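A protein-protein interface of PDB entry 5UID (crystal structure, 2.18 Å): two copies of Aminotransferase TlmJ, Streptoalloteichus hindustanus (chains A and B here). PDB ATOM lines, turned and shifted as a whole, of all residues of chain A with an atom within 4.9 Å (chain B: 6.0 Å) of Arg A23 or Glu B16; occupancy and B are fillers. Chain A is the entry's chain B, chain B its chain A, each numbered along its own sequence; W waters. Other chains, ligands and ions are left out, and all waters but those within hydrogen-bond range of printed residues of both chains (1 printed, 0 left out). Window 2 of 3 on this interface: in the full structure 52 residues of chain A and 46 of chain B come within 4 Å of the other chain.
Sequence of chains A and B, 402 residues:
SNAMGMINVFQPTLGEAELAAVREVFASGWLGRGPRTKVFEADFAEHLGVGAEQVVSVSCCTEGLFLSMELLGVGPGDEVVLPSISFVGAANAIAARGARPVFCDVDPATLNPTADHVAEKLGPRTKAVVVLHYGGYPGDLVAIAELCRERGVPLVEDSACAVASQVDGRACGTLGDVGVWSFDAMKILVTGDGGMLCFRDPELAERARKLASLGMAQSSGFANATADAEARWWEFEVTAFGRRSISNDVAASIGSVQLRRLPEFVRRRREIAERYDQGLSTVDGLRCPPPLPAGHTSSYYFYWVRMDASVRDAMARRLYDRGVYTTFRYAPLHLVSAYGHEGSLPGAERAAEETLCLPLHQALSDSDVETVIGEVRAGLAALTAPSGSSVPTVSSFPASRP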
ATOM      1  N   LEU A  19      -9.326  29.533   3.193  1.00  0.00           N
ATOM      2  CA  LEU A  19      -9.475  28.195   2.631  1.00  0.00           C
ATOM      3  C   LEU A  19      -9.803  27.178   3.717  1.00  0.00           C
ATOM      4  O   LEU A  19     -10.619  26.274   3.506  1.00  0.00           O
ATOM      5  CB  LEU A  19      -8.202  27.792   1.885  1.00  0.00           C
ATOM      6  CG  LEU A  19      -8.330  26.603   0.931  1.00  0.00           C
ATOM      7  CD1 LEU A  19      -9.208  26.971  -0.261  1.00  0.00           C
ATOM      8  CD2 LEU A  19      -6.962  26.126   0.473  1.00  0.00           C
ATOM      9  N   ALA A  20      -9.179  27.314   4.892  1.00  0.00           N
ATOM     10  CA  ALA A  20      -9.469  26.400   5.992  1.00  0.00           C
ATOM     11  C   ALA A  20     -10.920  26.522   6.445  1.00  0.00           C
ATOM     12  O   ALA A  20     -11.543  25.525   6.829  1.00  0.00           O
ATOM     13  CB  ALA A  20      -8.514  26.663   7.156  1.00  0.00           C
ATOM     14  N   ALA A  21     -11.475  27.737   6.407  1.00  0.00           N
ATOM     15  CA  ALA A  21     -12.890  27.911   6.721  1.00  0.00           C
ATOM     16  C   ALA A  21     -13.770  27.221   5.686  1.00  0.00           C
ATOM     17  O   ALA A  21     -14.754  26.562   6.040  1.00  0.00           O
ATOM     18  CB  ALA A  21     -13.228  29.399   6.813  1.00  0.00           C
ATOM     19  N   VAL A  22     -13.435  27.368   4.401  1.00  0.00           N
ATOM     20  CA  VAL A  22     -14.177  26.675   3.351  1.00  0.00           C
ATOM     21  C   VAL A  22     -14.106  25.166   3.557  1.00  0.00           C
ATOM     22  O   VAL A  22     -15.102  24.453   3.386  1.00  0.00           O
ATOM     23  CB  VAL A  22     -13.641  27.083   1.966  1.00  0.00           C
ATOM     24  CG1 VAL A  22     -14.403  26.356   0.859  1.00  0.00           C
ATOM     25  CG2 VAL A  22     -13.731  28.588   1.786  1.00  0.00           C
ATOM     26  N   ARG A  23     -12.929  24.662   3.938  1.00  0.00           N
ATOM     27  CA  ARG A  23     -12.758  23.227   4.151  1.00  0.00           C
ATOM     28  C   ARG A  23     -13.753  22.692   5.172  1.00  0.00           C
ATOM     29  O   ARG A  23     -14.371  21.640   4.956  1.00  0.00           O
ATOM     30  CB  ARG A  23     -11.325  22.931   4.599  1.00  0.00           C
ATOM     31  CG  ARG A  23     -11.072  21.469   4.927  1.00  0.00           C
ATOM     32  CD  ARG A  23      -9.650  21.245   5.415  1.00  0.00           C
ATOM     33  NE  ARG A  23      -8.658  21.611   4.409  1.00  0.00           N
ATOM     34  CZ  ARG A  23      -8.244  20.802   3.439  1.00  0.00           C
ATOM     35  NH1 ARG A  23      -8.738  19.574   3.340  1.00  0.00           N
ATOM     36  NH2 ARG A  23      -7.336  21.219   2.568  1.00  0.00           N
ATOM     37  N   GLU A  24     -13.927  23.403   6.289  1.00  0.00           N
ATOM     38  CA  GLU A  24     -14.866  22.951   7.309  1.00  0.00           C
ATOM     39  C   GLU A  24     -16.294  22.938   6.777  1.00  0.00           C
ATOM     40  O   GLU A  24     -17.074  22.033   7.094  1.00  0.00           O
ATOM     41  CB  GLU A  24     -14.759  23.836   8.554  1.00  0.00           C
ATOM     42  CG  GLU A  24     -13.459  23.649   9.327  1.00  0.00           C
ATOM     43  CD  GLU A  24     -13.373  24.527  10.568  1.00  0.00           C
ATOM     44  OE1 GLU A  24     -14.116  25.528  10.647  1.00  0.00           O
ATOM     45  OE2 GLU A  24     -12.561  24.209  11.464  1.00  0.00           O
ATOM     46  N   VAL A  25     -16.653  23.925   5.956  1.00  0.00           N
ATOM     47  CA  VAL A  25     -18.007  23.971   5.419  1.00  0.00           C
ATOM     48  C   VAL A  25     -18.242  22.817   4.450  1.00  0.00           C
ATOM     49  O   VAL A  25     -19.286  22.157   4.496  1.00  0.00           O
ATOM     50  CB  VAL A  25     -18.279  25.335   4.761  1.00  0.00           C
ATOM     51  CG1 VAL A  25     -19.642  25.328   4.088  1.00  0.00           C
ATOM     52  CG2 VAL A  25     -18.198  26.443   5.797  1.00  0.00           C
ATOM     53  N   PHE A  26     -17.282  22.560   3.554  1.00  0.00           N
ATOM     54  CA  PHE A  26     -17.386  21.407   2.663  1.00  0.00           C
ATOM     55  C   PHE A  26     -17.547  20.119   3.460  1.00  0.00           C
ATOM     56  O   PHE A  26     -18.432  19.303   3.178  1.00  0.00           O
ATOM     57  CB  PHE A  26     -16.150  21.305   1.765  1.00  0.00           C
ATOM     58  CG  PHE A  26     -16.093  22.332   0.671  1.00  0.00           C
ATOM     59  CD1 PHE A  26     -17.109  23.258   0.504  1.00  0.00           C
ATOM     60  CD2 PHE A  26     -15.018  22.358  -0.205  1.00  0.00           C
ATOM     61  CE1 PHE A  26     -17.048  24.197  -0.508  1.00  0.00           C
ATOM     62  CE2 PHE A  26     -14.949  23.294  -1.216  1.00  0.00           C
ATOM     63  CZ  PHE A  26     -15.967  24.213  -1.371  1.00  0.00           C
ATOM     64  N   ALA A  27     -16.696  19.925   4.468  1.00  0.00           N
ATOM     65  CA  ALA A  27     -16.732  18.693   5.245  1.00  0.00           C
ATOM     66  C   ALA A  27     -18.025  18.560   6.038  1.00  0.00           C
ATOM     67  O   ALA A  27     -18.464  17.439   6.317  1.00  0.00           O
ATOM     68  CB  ALA A  27     -15.519  18.626   6.177  1.00  0.00           C
ATOM     69  N   LEU B  14     -18.317  18.063  -1.892  1.00  0.00           N
ATOM     70  CA  LEU B  14     -17.206  18.908  -2.308  1.00  0.00           C
ATOM     71  C   LEU B  14     -16.012  18.612  -1.412  1.00  0.00           C
ATOM     72  O   LEU B  14     -16.156  18.533  -0.187  1.00  0.00           O
ATOM     73  CB  LEU B  14     -17.577  20.394  -2.238  1.00  0.00           C
ATOM     74  CG  LEU B  14     -18.458  20.959  -3.365  1.00  0.00           C
ATOM     75  CD1 LEU B  14     -19.900  20.470  -3.283  1.00  0.00           C
ATOM     76  CD2 LEU B  14     -18.411  22.480  -3.371  1.00  0.00           C
ATOM     77  N   GLY B  15     -14.841  18.443  -2.023  1.00  0.00           N
ATOM     78  CA  GLY B  15     -13.665  18.039  -1.278  1.00  0.00           C
ATOM     79  C   GLY B  15     -12.368  18.677  -1.737  1.00  0.00           C
ATOM     80  O   GLY B  15     -12.327  19.877  -2.028  1.00  0.00           O
ATOM     81  N   GLU B  16     -11.303  17.872  -1.812  1.00  0.00           N
ATOM     82  CA  GLU B  16      -9.971  18.414  -2.068  1.00  0.00           C
ATOM     83  C   GLU B  16      -9.863  19.030  -3.458  1.00  0.00           C
ATOM     84  O   GLU B  16      -9.222  20.076  -3.627  1.00  0.00           O
ATOM     85  CB  GLU B  16      -8.915  17.323  -1.885  1.00  0.00           C
ATOM     86  CG  GLU B  16      -8.711  16.889  -0.442  1.00  0.00           C
ATOM     87  CD  GLU B  16      -8.090  17.974   0.423  1.00  0.00           C
ATOM     88  OE1 GLU B  16      -7.522  18.940  -0.131  1.00  0.00           O
ATOM     89  OE2 GLU B  16      -8.169  17.857   1.664  1.00  0.00           O
ATOM     90  N   ALA B  17     -10.471  18.400  -4.466  1.00  0.00           N
ATOM     91  CA  ALA B  17     -10.377  18.934  -5.822  1.00  0.00           C
ATOM     92  C   ALA B  17     -11.064  20.290  -5.929  1.00  0.00           C
ATOM     93  O   ALA B  17     -10.555  21.201  -6.591  1.00  0.00           O
ATOM     94  CB  ALA B  17     -10.971  17.944  -6.824  1.00  0.00           C
ATOM     95  N   GLU B  18     -12.219  20.445  -5.276  1.00  0.00           N
ATOM     96  CA  GLU B  18     -12.887  21.743  -5.258  1.00  0.00           C
ATOM     97  C   GLU B  18     -12.097  22.758  -4.440  1.00  0.00           C
ATOM     98  O   GLU B  18     -12.054  23.945  -4.785  1.00  0.00           O
ATOM     99  CB  GLU B  18     -14.308  21.599  -4.711  1.00  0.00           C
ATOM    100  CG  GLU B  18     -15.283  20.867  -5.632  1.00  0.00           C
ATOM    101  CD  GLU B  18     -15.142  19.351  -5.588  1.00  0.00           C
ATOM    102  OE1 GLU B  18     -14.315  18.841  -4.802  1.00  0.00           O
ATOM    103  OE2 GLU B  18     -15.867  18.667  -6.343  1.00  0.00           O
ATOM    104  N   LEU B  19     -11.465  22.310  -3.350  1.00  0.00           N
ATOM    105  CA  LEU B  19     -10.644  23.213  -2.547  1.00  0.00           C
ATOM    106  C   LEU B  19      -9.440  23.711  -3.333  1.00  0.00           C
ATOM    107  O   LEU B  19      -9.082  24.891  -3.249  1.00  0.00           O
ATOM    108  CB  LEU B  19     -10.183  22.514  -1.268  1.00  0.00           C
ATOM    109  CG  LEU B  19     -11.184  22.405  -0.120  1.00  0.00           C
ATOM    110  CD1 LEU B  19     -10.657  21.449   0.940  1.00  0.00           C
ATOM    111  CD2 LEU B  19     -11.466  23.780   0.478  1.00  0.00           C
ATOM    112  N   ALA B  20      -8.802  22.824  -4.099  1.00  0.00           N
ATOM    113  CA  ALA B  20      -7.638  23.226  -4.883  1.00  0.00           C
ATOM    114  C   ALA B  20      -8.012  24.281  -5.915  1.00  0.00           C
ATOM    115  O   ALA B  20      -7.227  25.197  -6.188  1.00  0.00           O
ATOM    116  CB  ALA B  20      -7.009  22.007  -5.557  1.00  0.00           C
ATOM    117  N   ALA B  21      -9.208  24.173  -6.498  1.00  0.00           N
ATOM    118  CA  ALA B  21      -9.675  25.203  -7.420  1.00  0.00           C
ATOM    119  C   ALA B  21      -9.850  26.535  -6.702  1.00  0.00           C
ATOM    120  O   ALA B  21      -9.413  27.581  -7.195  1.00  0.00           O
ATOM    121  CB  ALA B  21     -10.984  24.768  -8.083  1.00  0.00           C
ATOM    122  N   ARG B  23      -8.329  27.447  -4.024  1.00  0.00           N
ATOM    123  CA  ARG B  23      -7.004  27.904  -3.618  1.00  0.00           C
ATOM    124  C   ARG B  23      -6.339  28.727  -4.715  1.00  0.00           C
ATOM    125  O   ARG B  23      -5.823  29.821  -4.460  1.00  0.00           O
ATOM    126  CB  ARG B  23      -6.129  26.707  -3.241  1.00  0.00           C
ATOM    127  CG  ARG B  23      -4.766  27.092  -2.678  1.00  0.00           C
ATOM    128  CD  ARG B  23      -3.875  25.877  -2.447  1.00  0.00           C
ATOM    129  NE  ARG B  23      -4.475  24.906  -1.534  1.00  0.00           N
ATOM    130  CZ  ARG B  23      -4.843  23.677  -1.884  1.00  0.00           C
ATOM    131  NH1 ARG B  23      -4.665  23.260  -3.130  1.00  0.00           N
ATOM    132  NH2 ARG B  23      -5.383  22.861  -0.985  1.00  0.00           N
HETATM  133  O   HOH W   1     -19.580  18.751   0.597  1.00  0.00           O
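Of the 9 printed residues of chain B, 5 touch a printed residue of chain A.
Printed residues of chain B that touch a printed residue of chain A: Leu B14, Glu B16, Glu B18, Leu B19 and Arg B23.
Printed residues of chain A that touch a printed residue of chain B: Leu A19, Val A22, Arg A23 and Phe A26.
Among the printed residues, Asp or Glu carboxylates within 4 Å of a Lys or Arg side-chain nitrogen of the other chain: Arg A23 with Glu B16 (2.5 Å).
Of chain B, only Glu B16 and Leu B19 come within 4 Å of Arg A23.
Printed residues of chain B within 4 Å of Phe A26: Leu B14 (3.4 Å), Glu B18 (3.9 Å) and Leu B19 (3.8 Å).
Ala A27 touches none of the printed residues of chain B.
Of the printed residues of chain A, Leu B14 touches Phe A26 (3.4 Å).
Of the printed residues of chain A, Glu B16 touches Arg A23.
Ala B21 touches none of the printed residues of chain A.
Of the printed residues of chain A, Arg B23 touches Leu A19 (3.4 Å).
The nearest printed residue of chain A that does not touch Glu B16 is Phe A26 (6.0 Å).
The nearest printed residue of chain A that does not touch Leu B19 is Ala A20 (6.1 Å).
N of Gly B15 sits at hydrogen-bond distance from OE1 of Glu B18 (2.9 Å).
Leu B19 touches its own counterpart, Leu A19.
Leu A19 touches Arg B23, and with the chains exchanged Arg A23 touches Leu B19.
Of the 8 pairs that touch across the chains among the printed residues, 3 have their exchanged pair printed and touching as well.
OE2 of Glu B16 is in salt-bridge range of NH1 of Arg A23.
Water W1 lies within hydrogen-bond range of the backbone NH (N) of Leu B14 (2.9 Å) and the backbone carbonyl oxygen (O) of Phe A26 (2.9 Å).
Leu B19 touches Leu A19.
NE of Arg B23 touches CD2 of Leu A19, 3.4 Å away.
Leu B19 touches Val A22 (CD2 to CG1, 3.9 Å).
CZ of Arg A23 touches CD1 of Leu B19 (3.5 Å).
Phe A26 touches Leu B14.
CB of Glu B18 touches CE2 of Phe A26, at 3.9 Å.
Leu B19 touches Phe A26 (CG to CD2, 3.8 Å).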
